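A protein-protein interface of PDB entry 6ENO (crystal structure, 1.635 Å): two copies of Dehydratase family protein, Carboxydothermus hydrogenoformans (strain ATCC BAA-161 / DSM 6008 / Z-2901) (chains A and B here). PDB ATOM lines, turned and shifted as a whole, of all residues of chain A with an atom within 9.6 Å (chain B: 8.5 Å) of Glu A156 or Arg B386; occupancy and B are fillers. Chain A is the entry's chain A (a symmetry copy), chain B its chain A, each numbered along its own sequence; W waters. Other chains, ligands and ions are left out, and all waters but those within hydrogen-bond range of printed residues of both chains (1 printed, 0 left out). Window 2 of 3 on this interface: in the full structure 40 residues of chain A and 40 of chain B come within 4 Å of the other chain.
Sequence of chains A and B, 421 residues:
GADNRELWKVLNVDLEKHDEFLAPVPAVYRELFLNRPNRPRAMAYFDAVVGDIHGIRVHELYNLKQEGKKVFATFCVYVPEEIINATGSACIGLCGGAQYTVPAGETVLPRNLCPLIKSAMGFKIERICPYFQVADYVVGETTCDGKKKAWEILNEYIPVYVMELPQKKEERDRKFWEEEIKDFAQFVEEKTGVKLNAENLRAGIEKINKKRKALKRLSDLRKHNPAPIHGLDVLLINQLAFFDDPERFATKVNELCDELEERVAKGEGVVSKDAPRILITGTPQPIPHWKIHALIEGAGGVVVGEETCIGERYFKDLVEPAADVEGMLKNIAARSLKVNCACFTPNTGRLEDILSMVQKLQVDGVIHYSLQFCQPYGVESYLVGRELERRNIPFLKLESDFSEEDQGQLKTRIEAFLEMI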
ATOM      1  N   THR A 107      26.096   3.107  16.028  1.00  0.00           N
ATOM      2  CA  THR A 107      26.011   2.876  14.596  1.00  0.00           C
ATOM      3  C   THR A 107      24.665   2.260  14.227  1.00  0.00           C
ATOM      4  O   THR A 107      24.263   2.336  13.059  1.00  0.00           O
ATOM      5  CB  THR A 107      27.185   2.011  14.123  1.00  0.00           C
ATOM      6  OG1 THR A 107      27.055   0.675  14.622  1.00  0.00           O
ATOM      7  CG2 THR A 107      28.512   2.597  14.628  1.00  0.00           C
ATOM      8  N   VAL A 108      23.918   1.726  15.202  1.00  0.00           N
ATOM      9  CA  VAL A 108      22.610   1.148  14.900  1.00  0.00           C
ATOM     10  C   VAL A 108      21.524   1.582  15.889  1.00  0.00           C
ATOM     11  O   VAL A 108      20.342   1.285  15.680  1.00  0.00           O
ATOM     12  CB  VAL A 108      22.698  -0.394  14.838  1.00  0.00           C
ATOM     13  CG1 VAL A 108      23.724  -0.810  13.813  1.00  0.00           C
ATOM     14  CG2 VAL A 108      23.007  -1.022  16.245  1.00  0.00           C
ATOM     15  N   MET A 121      25.478  -3.281  22.886  1.00  0.00           N
ATOM     16  CA  MET A 121      25.349  -3.458  21.445  1.00  0.00           C
ATOM     17  C   MET A 121      26.701  -3.299  20.778  1.00  0.00           C
ATOM     18  O   MET A 121      27.047  -4.039  19.849  1.00  0.00           O
ATOM     19  CB  MET A 121      24.355  -2.443  20.889  1.00  0.00           C
ATOM     20  CG  MET A 121      24.099  -2.539  19.405  1.00  0.00           C
ATOM     21  SD  MET A 121      23.259  -4.011  18.840  1.00  0.00           S
ATOM     22  CE  MET A 121      21.567  -3.561  19.214  1.00  0.00           C
ATOM     23  N   LYS A 124      29.126  -6.358  21.020  1.00  0.00           N
ATOM     24  CA  LYS A 124      28.880  -7.491  20.131  1.00  0.00           C
ATOM     25  C   LYS A 124      29.101  -7.123  18.671  1.00  0.00           C
ATOM     26  O   LYS A 124      29.707  -7.886  17.917  1.00  0.00           O
ATOM     27  CB  LYS A 124      27.451  -8.020  20.326  1.00  0.00           C
ATOM     28  CG  LYS A 124      27.043  -9.138  19.342  1.00  0.00           C
ATOM     29  CD  LYS A 124      27.955 -10.371  19.426  1.00  0.00           C
ATOM     30  CE  LYS A 124      28.081 -11.068  18.081  1.00  0.00           C
ATOM     31  NZ  LYS A 124      29.128 -12.116  18.122  1.00  0.00           N
ATOM     32  N   ILE A 125      28.606  -5.970  18.237  1.00  0.00           N
ATOM     33  CA  ILE A 125      28.604  -5.707  16.811  1.00  0.00           C
ATOM     34  C   ILE A 125      30.040  -5.526  16.296  1.00  0.00           C
ATOM     35  O   ILE A 125      30.344  -5.897  15.155  1.00  0.00           O
ATOM     36  CB  ILE A 125      27.689  -4.499  16.523  1.00  0.00           C
ATOM     37  CG1 ILE A 125      27.332  -4.439  15.040  1.00  0.00           C
ATOM     38  CG2 ILE A 125      28.366  -3.219  17.009  1.00  0.00           C
ATOM     39  CD1 ILE A 125      25.893  -3.917  14.745  1.00  0.00           C
ATOM     40  N   VAL A 138      21.501 -15.036  23.254  1.00  0.00           N
ATOM     41  CA  VAL A 138      21.058 -13.962  24.140  1.00  0.00           C
ATOM     42  C   VAL A 138      19.608 -14.239  24.515  1.00  0.00           C
ATOM     43  O   VAL A 138      18.782 -14.604  23.664  1.00  0.00           O
ATOM     44  CB  VAL A 138      21.168 -12.559  23.510  1.00  0.00           C
ATOM     45  CG1 VAL A 138      20.450 -11.540  24.372  1.00  0.00           C
ATOM     46  CG2 VAL A 138      22.645 -12.140  23.349  1.00  0.00           C
ATOM     47  N   LYS A 149      13.309  -2.811  21.928  1.00  0.00           N
ATOM     48  CA  LYS A 149      13.457  -2.586  20.498  1.00  0.00           C
ATOM     49  C   LYS A 149      14.881  -2.894  20.031  1.00  0.00           C
ATOM     50  O   LYS A 149      15.075  -3.224  18.859  1.00  0.00           O
ATOM     51  CB  LYS A 149      13.049  -1.138  20.147  1.00  0.00           C
ATOM     52  CG  LYS A 149      11.604  -0.786  20.600  1.00  0.00           C
ATOM     53  CD  LYS A 149      10.556  -1.735  19.957  1.00  0.00           C
ATOM     54  CE  LYS A 149      10.372  -1.485  18.470  1.00  0.00           C
ATOM     55  NZ  LYS A 149       9.349  -2.432  17.881  1.00  0.00           N
ATOM     56  N   ALA A 150      15.859  -2.841  20.931  1.00  0.00           N
ATOM     57  CA  ALA A 150      17.233  -3.159  20.545  1.00  0.00           C
ATOM     58  C   ALA A 150      17.402  -4.639  20.209  1.00  0.00           C
ATOM     59  O   ALA A 150      18.177  -4.973  19.304  1.00  0.00           O
ATOM     60  CB  ALA A 150      18.192  -2.753  21.653  1.00  0.00           C
ATOM     61  N   TRP A 151      16.664  -5.531  20.888  1.00  0.00           N
ATOM     62  CA  TRP A 151      16.775  -6.964  20.596  1.00  0.00           C
ATOM     63  C   TRP A 151      16.462  -7.261  19.131  1.00  0.00           C
ATOM     64  O   TRP A 151      17.029  -8.196  18.544  1.00  0.00           O
ATOM     65  CB  TRP A 151      15.848  -7.804  21.492  1.00  0.00           C
ATOM     66  CG  TRP A 151      15.900  -7.556  22.975  1.00  0.00           C
ATOM     67  CD1 TRP A 151      14.816  -7.477  23.831  1.00  0.00           C
ATOM     68  CD2 TRP A 151      17.063  -7.372  23.803  1.00  0.00           C
ATOM     69  NE1 TRP A 151      15.248  -7.241  25.114  1.00  0.00           N
ATOM     70  CE2 TRP A 151      16.614  -7.187  25.127  1.00  0.00           C
ATOM     71  CE3 TRP A 151      18.443  -7.351  23.557  1.00  0.00           C
ATOM     72  CZ2 TRP A 151      17.487  -6.971  26.192  1.00  0.00           C
ATOM     73  CZ3 TRP A 151      19.297  -7.143  24.617  1.00  0.00           C
ATOM     74  CH2 TRP A 151      18.820  -6.938  25.911  1.00  0.00           C
ATOM     75  N   GLU A 152      15.524  -6.520  18.540  1.00  0.00           N
ATOM     76  CA  GLU A 152      15.154  -6.759  17.145  1.00  0.00           C
ATOM     77  C   GLU A 152      16.344  -6.554  16.230  1.00  0.00           C
ATOM     78  O   GLU A 152      16.449  -7.202  15.183  1.00  0.00           O
ATOM     79  CB  GLU A 152      14.001  -5.839  16.740  1.00  0.00           C
ATOM     80  CG  GLU A 152      12.734  -5.940  17.616  1.00  0.00           C
ATOM     81  CD  GLU A 152      11.675  -4.938  17.257  1.00  0.00           C
ATOM     82  OE1 GLU A 152      11.880  -4.088  16.334  1.00  0.00           O
ATOM     83  OE2 GLU A 152      10.631  -5.010  17.902  1.00  0.00           O
ATOM     84  N   ILE A 153      17.231  -5.633  16.603  1.00  0.00           N
ATOM     85  CA  ILE A 153      18.441  -5.334  15.840  1.00  0.00           C
ATOM     86  C   ILE A 153      19.545  -6.323  16.183  1.00  0.00           C
ATOM     87  O   ILE A 153      20.261  -6.802  15.292  1.00  0.00           O
ATOM     88  CB  ILE A 153      18.900  -3.897  16.142  1.00  0.00           C
ATOM     89  CG1 ILE A 153      17.891  -2.889  15.593  1.00  0.00           C
ATOM     90  CG2 ILE A 153      20.267  -3.548  15.509  1.00  0.00           C
ATOM     91  CD1 ILE A 153      18.059  -1.527  16.188  1.00  0.00           C
ATOM     92  N   LEU A 154      19.741  -6.570  17.480  1.00  0.00           N
ATOM     93  CA  LEU A 154      20.806  -7.469  17.942  1.00  0.00           C
ATOM     94  C   LEU A 154      20.639  -8.880  17.385  1.00  0.00           C
ATOM     95  O   LEU A 154      21.627  -9.570  17.106  1.00  0.00           O
ATOM     96  CB  LEU A 154      20.828  -7.506  19.477  1.00  0.00           C
ATOM     97  CG  LEU A 154      21.900  -8.404  20.107  1.00  0.00           C
ATOM     98  CD1 LEU A 154      23.286  -7.911  19.732  1.00  0.00           C
ATOM     99  CD2 LEU A 154      21.675  -8.417  21.583  1.00  0.00           C
ATOM    100  N   ASN A 155      19.390  -9.322  17.233  1.00  0.00           N
ATOM    101  CA  ASN A 155      19.085 -10.667  16.750  1.00  0.00           C
ATOM    102  C   ASN A 155      19.759 -10.949  15.411  1.00  0.00           C
ATOM    103  O   ASN A 155      19.976 -12.114  15.072  1.00  0.00           O
ATOM    104  CB  ASN A 155      17.562 -10.817  16.656  1.00  0.00           C
ATOM    105  CG  ASN A 155      17.134 -12.195  16.250  1.00  0.00           C
ATOM    106  OD1 ASN A 155      17.413 -13.171  16.933  1.00  0.00           O
ATOM    107  ND2 ASN A 155      16.451 -12.286  15.111  1.00  0.00           N
ATOM    108  N   GLU A 156      20.104  -9.901  14.657  1.00  0.00           N
ATOM    109  CA  GLU A 156      20.806 -10.059  13.378  1.00  0.00           C
ATOM    110  C   GLU A 156      22.236 -10.576  13.554  1.00  0.00           C
ATOM    111  O   GLU A 156      22.780 -11.190  12.623  1.00  0.00           O
ATOM    112  CB  GLU A 156      20.825  -8.717  12.626  1.00  0.00           C
ATOM    113  CG  GLU A 156      19.620  -8.476  11.721  1.00  0.00           C
ATOM    114  CD  GLU A 156      19.114  -7.023  11.749  1.00  0.00           C
ATOM    115  OE1 GLU A 156      17.881  -6.833  11.625  1.00  0.00           O
ATOM    116  OE2 GLU A 156      19.935  -6.078  11.902  1.00  0.00           O
ATOM    117  N   TYR A 157      22.859 -10.336  14.725  1.00  0.00           N
ATOM    118  CA  TYR A 157      24.248 -10.700  15.000  1.00  0.00           C
ATOM    119  C   TYR A 157      24.428 -11.880  15.956  1.00  0.00           C
ATOM    120  O   TYR A 157      25.508 -12.503  15.956  1.00  0.00           O
ATOM    121  CB  TYR A 157      24.970  -9.467  15.557  1.00  0.00           C
ATOM    122  CG  TYR A 157      24.859  -8.377  14.547  1.00  0.00           C
ATOM    123  CD1 TYR A 157      25.689  -8.387  13.427  1.00  0.00           C
ATOM    124  CD2 TYR A 157      23.864  -7.394  14.629  1.00  0.00           C
ATOM    125  CE1 TYR A 157      25.575  -7.422  12.434  1.00  0.00           C
ATOM    126  CE2 TYR A 157      23.760  -6.429  13.639  1.00  0.00           C
ATOM    127  CZ  TYR A 157      24.623  -6.448  12.553  1.00  0.00           C
ATOM    128  OH  TYR A 157      24.498  -5.512  11.563  1.00  0.00           O
ATOM    129  N   ILE A 158      23.416 -12.207  16.753  1.00  0.00           N
ATOM    130  CA  ILE A 158      23.424 -13.350  17.666  1.00  0.00           C
ATOM    131  C   ILE A 158      21.958 -13.691  17.938  1.00  0.00           C
ATOM    132  O   ILE A 158      21.139 -12.772  18.039  1.00  0.00           O
ATOM    133  CB  ILE A 158      24.229 -13.039  18.940  1.00  0.00           C
ATOM    134  CG1 ILE A 158      24.316 -14.251  19.867  1.00  0.00           C
ATOM    135  CG2 ILE A 158      23.676 -11.817  19.688  1.00  0.00           C
ATOM    136  CD1 ILE A 158      25.281 -14.079  20.993  1.00  0.00           C
ATOM    137  N   PRO A 159      21.562 -14.963  18.006  1.00  0.00           N
ATOM    138  CA  PRO A 159      20.138 -15.258  18.233  1.00  0.00           C
ATOM    139  C   PRO A 159      19.673 -14.756  19.599  1.00  0.00           C
ATOM    140  O   PRO A 159      20.281 -15.061  20.633  1.00  0.00           O
ATOM    141  CB  PRO A 159      20.054 -16.781  18.143  1.00  0.00           C
ATOM    142  CG  PRO A 159      21.245 -17.188  17.333  1.00  0.00           C
ATOM    143  CD  PRO A 159      22.329 -16.188  17.710  1.00  0.00           C
ATOM    144  N   VAL A 160      18.560 -13.999  19.583  1.00  0.00           N
ATOM    145  CA  VAL A 160      17.952 -13.430  20.782  1.00  0.00           C
ATOM    146  C   VAL A 160      16.599 -14.106  20.981  1.00  0.00           C
ATOM    147  O   VAL A 160      15.728 -14.024  20.100  1.00  0.00           O
ATOM    148  CB  VAL A 160      17.755 -11.901  20.693  1.00  0.00           C
ATOM    149  CG1 VAL A 160      17.087 -11.388  21.941  1.00  0.00           C
ATOM    150  CG2 VAL A 160      19.081 -11.126  20.445  1.00  0.00           C
ATOM    151  N   LEU B 351       6.017  -2.011   8.819  1.00  0.00           N
ATOM    152  CA  LEU B 351       6.769  -1.833   7.588  1.00  0.00           C
ATOM    153  C   LEU B 351       5.932  -2.180   6.357  1.00  0.00           C
ATOM    154  O   LEU B 351       5.959  -1.458   5.366  1.00  0.00           O
ATOM    155  CB  LEU B 351       8.064  -2.658   7.616  1.00  0.00           C
ATOM    156  CG  LEU B 351       9.379  -1.885   7.574  1.00  0.00           C
ATOM    157  CD1 LEU B 351      10.544  -2.864   7.734  1.00  0.00           C
ATOM    158  CD2 LEU B 351       9.550  -1.083   6.318  1.00  0.00           C
ATOM    159  N   GLU B 380      13.098   1.858  16.409  1.00  0.00           N
ATOM    160  CA  GLU B 380      12.571   1.114  15.263  1.00  0.00           C
ATOM    161  C   GLU B 380      12.874   1.807  13.924  1.00  0.00           C
ATOM    162  O   GLU B 380      12.845   1.150  12.869  1.00  0.00           O
ATOM    163  CB  GLU B 380      11.052   0.910  15.430  1.00  0.00           C
ATOM    164  CG  GLU B 380      10.429   0.026  14.359  1.00  0.00           C
ATOM    165  CD  GLU B 380       8.953  -0.341  14.620  1.00  0.00           C
ATOM    166  OE1 GLU B 380       8.637  -1.048  15.625  1.00  0.00           O
ATOM    167  OE2 GLU B 380       8.098   0.018  13.797  1.00  0.00           O
ATOM    168  N   SER B 381      13.192   3.105  13.944  1.00  0.00           N
ATOM    169  CA  SER B 381      13.495   3.809  12.697  1.00  0.00           C
ATOM    170  C   SER B 381      14.662   3.190  11.944  1.00  0.00           C
ATOM    171  O   SER B 381      14.793   3.393  10.730  1.00  0.00           O
ATOM    172  CB  SER B 381      13.809   5.288  12.997  1.00  0.00           C
ATOM    173  OG  SER B 381      15.088   5.396  13.595  1.00  0.00           O
ATOM    174  N   TYR B 382      15.575   2.525  12.643  1.00  0.00           N
ATOM    175  CA  TYR B 382      16.719   1.924  11.963  1.00  0.00           C
ATOM    176  C   TYR B 382      16.285   0.813  11.008  1.00  0.00           C
ATOM    177  O   TYR B 382      16.707   0.780   9.846  1.00  0.00           O
ATOM    178  CB  TYR B 382      17.706   1.395  13.004  1.00  0.00           C
ATOM    179  CG  TYR B 382      18.831   0.600  12.392  1.00  0.00           C
ATOM    180  CD1 TYR B 382      19.939   1.233  11.857  1.00  0.00           C
ATOM    181  CD2 TYR B 382      18.777  -0.799  12.345  1.00  0.00           C
ATOM    182  CE1 TYR B 382      20.962   0.490  11.289  1.00  0.00           C
ATOM    183  CE2 TYR B 382      19.794  -1.548  11.764  1.00  0.00           C
ATOM    184  CZ  TYR B 382      20.881  -0.895  11.246  1.00  0.00           C
ATOM    185  OH  TYR B 382      21.891  -1.637  10.669  1.00  0.00           O
ATOM    186  N   LEU B 383      15.443  -0.119  11.479  1.00  0.00           N
ATOM    187  CA  LEU B 383      15.011  -1.217  10.621  1.00  0.00           C
ATOM    188  C   LEU B 383      14.101  -0.716   9.498  1.00  0.00           C
ATOM    189  O   LEU B 383      14.130  -1.257   8.376  1.00  0.00           O
ATOM    190  CB  LEU B 383      14.310  -2.277  11.468  1.00  0.00           C
ATOM    191  CG  LEU B 383      15.265  -3.174  12.261  1.00  0.00           C
ATOM    192  CD1 LEU B 383      14.407  -4.034  13.229  1.00  0.00           C
ATOM    193  CD2 LEU B 383      16.166  -4.021  11.362  1.00  0.00           C
ATOM    194  N   VAL B 384      13.259   0.269   9.802  1.00  0.00           N
ATOM    195  CA  VAL B 384      12.380   0.871   8.794  1.00  0.00           C
ATOM    196  C   VAL B 384      13.200   1.513   7.679  1.00  0.00           C
ATOM    197  O   VAL B 384      12.996   1.233   6.489  1.00  0.00           O
ATOM    198  CB  VAL B 384      11.436   1.891   9.454  1.00  0.00           C
ATOM    199  CG1 VAL B 384      10.675   2.657   8.419  1.00  0.00           C
ATOM    200  CG2 VAL B 384      10.465   1.179  10.389  1.00  0.00           C
ATOM    201  N   GLY B 385      14.144   2.376   8.043  1.00  0.00           N
ATOM    202  CA  GLY B 385      14.974   3.004   7.029  1.00  0.00           C
ATOM    203  C   GLY B 385      15.749   2.004   6.196  1.00  0.00           C
ATOM    204  O   GLY B 385      15.902   2.178   4.986  1.00  0.00           O
ATOM    205  N   ARG B 386      16.252   0.939   6.826  1.00  0.00           N
ATOM    206  CA  ARG B 386      17.050  -0.021   6.079  1.00  0.00           C
ATOM    207  C   ARG B 386      16.243  -0.639   4.945  1.00  0.00           C
ATOM    208  O   ARG B 386      16.753  -0.810   3.838  1.00  0.00           O
ATOM    209  CB  ARG B 386      17.588  -1.113   7.010  1.00  0.00           C
ATOM    210  CG  ARG B 386      18.460  -2.136   6.264  1.00  0.00           C
ATOM    211  CD  ARG B 386      18.966  -3.280   7.146  1.00  0.00           C
ATOM    212  NE  ARG B 386      17.895  -4.206   7.529  1.00  0.00           N
ATOM    213  CZ  ARG B 386      18.093  -5.338   8.201  1.00  0.00           C
ATOM    214  NH1 ARG B 386      17.063  -6.118   8.498  1.00  0.00           N
ATOM    215  NH2 ARG B 386      19.327  -5.698   8.554  1.00  0.00           N
ATOM    216  N   GLU B 387      14.981  -1.009   5.207  1.00  0.00           N
ATOM    217  CA  GLU B 387      14.206  -1.675   4.167  1.00  0.00           C
ATOM    218  C   GLU B 387      13.777  -0.685   3.101  1.00  0.00           C
ATOM    219  O   GLU B 387      13.793  -1.003   1.909  1.00  0.00           O
ATOM    220  CB  GLU B 387      12.993  -2.382   4.773  1.00  0.00           C
ATOM    221  CG  GLU B 387      12.026  -3.037   3.763  1.00  0.00           C
ATOM    222  CD  GLU B 387      12.606  -4.165   2.903  1.00  0.00           C
ATOM    223  OE1 GLU B 387      13.717  -4.718   3.154  1.00  0.00           O
ATOM    224  OE2 GLU B 387      11.911  -4.510   1.922  1.00  0.00           O
ATOM    225  N   LEU B 388      13.431   0.534   3.505  1.00  0.00           N
ATOM    226  CA  LEU B 388      13.102   1.547   2.515  1.00  0.00           C
ATOM    227  C   LEU B 388      14.310   1.867   1.627  1.00  0.00           C
ATOM    228  O   LEU B 388      14.185   1.965   0.400  1.00  0.00           O
ATOM    229  CB  LEU B 388      12.568   2.794   3.226  1.00  0.00           C
ATOM    230  CG  LEU B 388      11.053   2.915   3.337  1.00  0.00           C
ATOM    231  CD1 LEU B 388      10.376   1.641   3.768  1.00  0.00           C
ATOM    232  CD2 LEU B 388      10.751   4.042   4.319  1.00  0.00           C
ATOM    233  N   GLU B 389      15.501   1.975   2.214  1.00  0.00           N
ATOM    234  CA  GLU B 389      16.673   2.293   1.405  1.00  0.00           C
ATOM    235  C   GLU B 389      17.092   1.102   0.549  1.00  0.00           C
ATOM    236  O   GLU B 389      17.499   1.285  -0.601  1.00  0.00           O
ATOM    237  CB  GLU B 389      17.810   2.781   2.305  1.00  0.00           C
ATOM    238  CG  GLU B 389      17.465   4.106   3.027  1.00  0.00           C
ATOM    239  CD  GLU B 389      18.682   4.776   3.647  1.00  0.00           C
ATOM    240  OE1 GLU B 389      18.930   5.967   3.340  1.00  0.00           O
ATOM    241  OE2 GLU B 389      19.401   4.100   4.425  1.00  0.00           O
ATOM    242  N   ARG B 390      16.954  -0.132   1.067  1.00  0.00           N
ATOM    243  CA  ARG B 390      17.176  -1.290   0.200  1.00  0.00           C
ATOM    244  C   ARG B 390      16.325  -1.176  -1.061  1.00  0.00           C
ATOM    245  O   ARG B 390      16.781  -1.501  -2.163  1.00  0.00           O
ATOM    246  CB  ARG B 390      16.872  -2.615   0.927  1.00  0.00           C
ATOM    247  CG  ARG B 390      17.005  -3.836  -0.018  1.00  0.00           C
ATOM    248  CD  ARG B 390      16.496  -5.116   0.607  1.00  0.00           C
ATOM    249  NE  ARG B 390      15.035  -5.221   0.565  1.00  0.00           N
ATOM    250  CZ  ARG B 390      14.336  -5.650  -0.489  1.00  0.00           C
ATOM    251  NH1 ARG B 390      14.937  -5.990  -1.625  1.00  0.00           N
ATOM    252  NH2 ARG B 390      13.020  -5.738  -0.413  1.00  0.00           N
ATOM    253  N   ARG B 391      15.087  -0.679  -0.928  1.00  0.00           N
ATOM    254  CA  ARG B 391      14.229  -0.490  -2.094  1.00  0.00           C
ATOM    255  C   ARG B 391      14.472   0.833  -2.805  1.00  0.00           C
ATOM    256  O   ARG B 391      13.715   1.163  -3.721  1.00  0.00           O
ATOM    257  CB  ARG B 391      12.757  -0.591  -1.693  1.00  0.00           C
ATOM    258  CG  ARG B 391      12.321  -1.992  -1.251  1.00  0.00           C
ATOM    259  CD  ARG B 391      11.016  -1.891  -0.494  1.00  0.00           C
ATOM    260  NE  ARG B 391      10.538  -3.177  -0.012  1.00  0.00           N
ATOM    261  CZ  ARG B 391       9.933  -4.080  -0.772  1.00  0.00           C
ATOM    262  NH1 ARG B 391       9.750  -3.846  -2.074  1.00  0.00           N
ATOM    263  NH2 ARG B 391       9.522  -5.214  -0.235  1.00  0.00           N
ATOM    264  N   ASN B 392      15.508   1.579  -2.421  1.00  0.00           N
ATOM    265  CA  ASN B 392      15.842   2.873  -3.031  1.00  0.00           C
ATOM    266  C   ASN B 392      14.661   3.847  -2.978  1.00  0.00           C
ATOM    267  O   ASN B 392      14.485   4.696  -3.864  1.00  0.00           O
ATOM    268  CB  ASN B 392      16.359   2.688  -4.466  1.00  0.00           C
ATOM    269  CG  ASN B 392      17.682   1.880  -4.518  1.00  0.00           C
ATOM    270  OD1 ASN B 392      18.654   2.215  -3.837  1.00  0.00           O
ATOM    271  ND2 ASN B 392      17.708   0.815  -5.323  1.00  0.00           N
ATOM    272  N   ILE B 393      13.857   3.752  -1.923  1.00  0.00           N
ATOM    273  CA  ILE B 393      12.868   4.790  -1.609  1.00  0.00           C
ATOM    274  C   ILE B 393      13.564   5.906  -0.836  1.00  0.00           C
ATOM    275  O   ILE B 393      14.123   5.655   0.236  1.00  0.00           O
ATOM    276  CB  ILE B 393      11.686   4.225  -0.810  1.00  0.00           C
ATOM    277  CG1 ILE B 393      10.930   3.182  -1.632  1.00  0.00           C
ATOM    278  CG2 ILE B 393      10.715   5.337  -0.380  1.00  0.00           C
ATOM    279  CD1 ILE B 393      10.053   2.249  -0.803  1.00  0.00           C
ATOM    280  N   PHE B 395      14.613   8.557   1.782  1.00  0.00           N
ATOM    281  CA  PHE B 395      14.338   8.448   3.212  1.00  0.00           C
ATOM    282  C   PHE B 395      15.082   9.527   3.990  1.00  0.00           C
ATOM    283  O   PHE B 395      16.304   9.668   3.861  1.00  0.00           O
ATOM    284  CB  PHE B 395      14.750   7.057   3.706  1.00  0.00           C
ATOM    285  CG  PHE B 395      14.365   6.774   5.114  1.00  0.00           C
ATOM    286  CD1 PHE B 395      13.060   6.439   5.431  1.00  0.00           C
ATOM    287  CD2 PHE B 395      15.306   6.795   6.118  1.00  0.00           C
ATOM    288  CE1 PHE B 395      12.703   6.154   6.726  1.00  0.00           C
ATOM    289  CE2 PHE B 395      14.947   6.490   7.417  1.00  0.00           C
ATOM    290  CZ  PHE B 395      13.650   6.171   7.716  1.00  0.00           C
ATOM    291  N   LYS B 397      15.372  10.929   8.043  1.00  0.00           N
ATOM    292  CA  LYS B 397      15.024  10.723   9.449  1.00  0.00           C
ATOM    293  C   LYS B 397      15.067  12.070  10.173  1.00  0.00           C
ATOM    294  O   LYS B 397      16.108  12.737  10.189  1.00  0.00           O
ATOM    295  CB  LYS B 397      15.953   9.710  10.116  1.00  0.00           C
ATOM    296  CG  LYS B 397      15.593   9.446  11.583  1.00  0.00           C
ATOM    297  CD  LYS B 397      16.024   8.051  12.039  1.00  0.00           C
ATOM    298  CE  LYS B 397      17.529   7.904  12.287  1.00  0.00           C
ATOM    299  NZ  LYS B 397      17.882   6.502  12.773  1.00  0.00           N
HETATM  300  O   HOH W   1      22.013  -4.499  10.971  1.00  0.00           O
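The side-chain carboxylate (OE1) of Glu B380 is in salt-bridge range of the side-chain amino group (NZ) of Lys A149 (2.7 Å).
The guanidinium group (NH1) of Arg B386 lies within salt-bridge range of the side-chain carboxylate (OE1) of Glu A156, 3.3 Å away.
The side-chain amino group (NZ) of Lys A149 is in salt-bridge range of the side-chain carboxylate (OE2) of Glu A152 (2.9 Å).
Tyr B382 touches Val A108.
Glu A152 touches Leu B383 (CB to CD1, 3.97 Å).
CG1 of Ile A153 touches CD2 of Tyr B382, at 3.96 Å.
Leu B383 touches Glu A156 (CD2 to OE1, 3.3 Å).
Glu A156 touches just these residues of chain B: Leu B383 (3.3 Å) and Arg B386 (3.3 Å).
Arg B386 touches just one residue of chain A: Glu A156.
No residue of chain A comes within 4 Å of Gly B385.
Of the printed residues of chain B, Ile A153 touches Tyr B382.
Of the printed residues of chain A, Tyr B382 touches Val A108 (3.7 Å) and Ile A153 (3.96 Å).
Of the printed residues of chain A, Leu B383 touches Glu A152 (3.97 Å) and Glu A156 (3.3 Å).
Printed residues of chain B within 4 Å of Val A108: Tyr B382.
Ile A125 touches none of the printed residues of chain B.
Printed residues of chain B that touch a printed residue of chain A: Glu B380, Tyr B382, Leu B383 and Arg B386.
Hydrophobic or aromatic side chains of chain A that line the printed part of chain B: Val A108 and Ile A153.
Among the printed residues, 6 pairs touch across the chains.
No position is printed for both chains.
Water W1 lies within hydrogen-bond range of the side-chain hydroxyl (OH) of Tyr A157 (2.7 Å), the side-chain carboxylate (OE2) of Glu A156 (2.8 Å) and the side-chain hydroxyl (OH) of Tyr B382 (2.9 Å).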
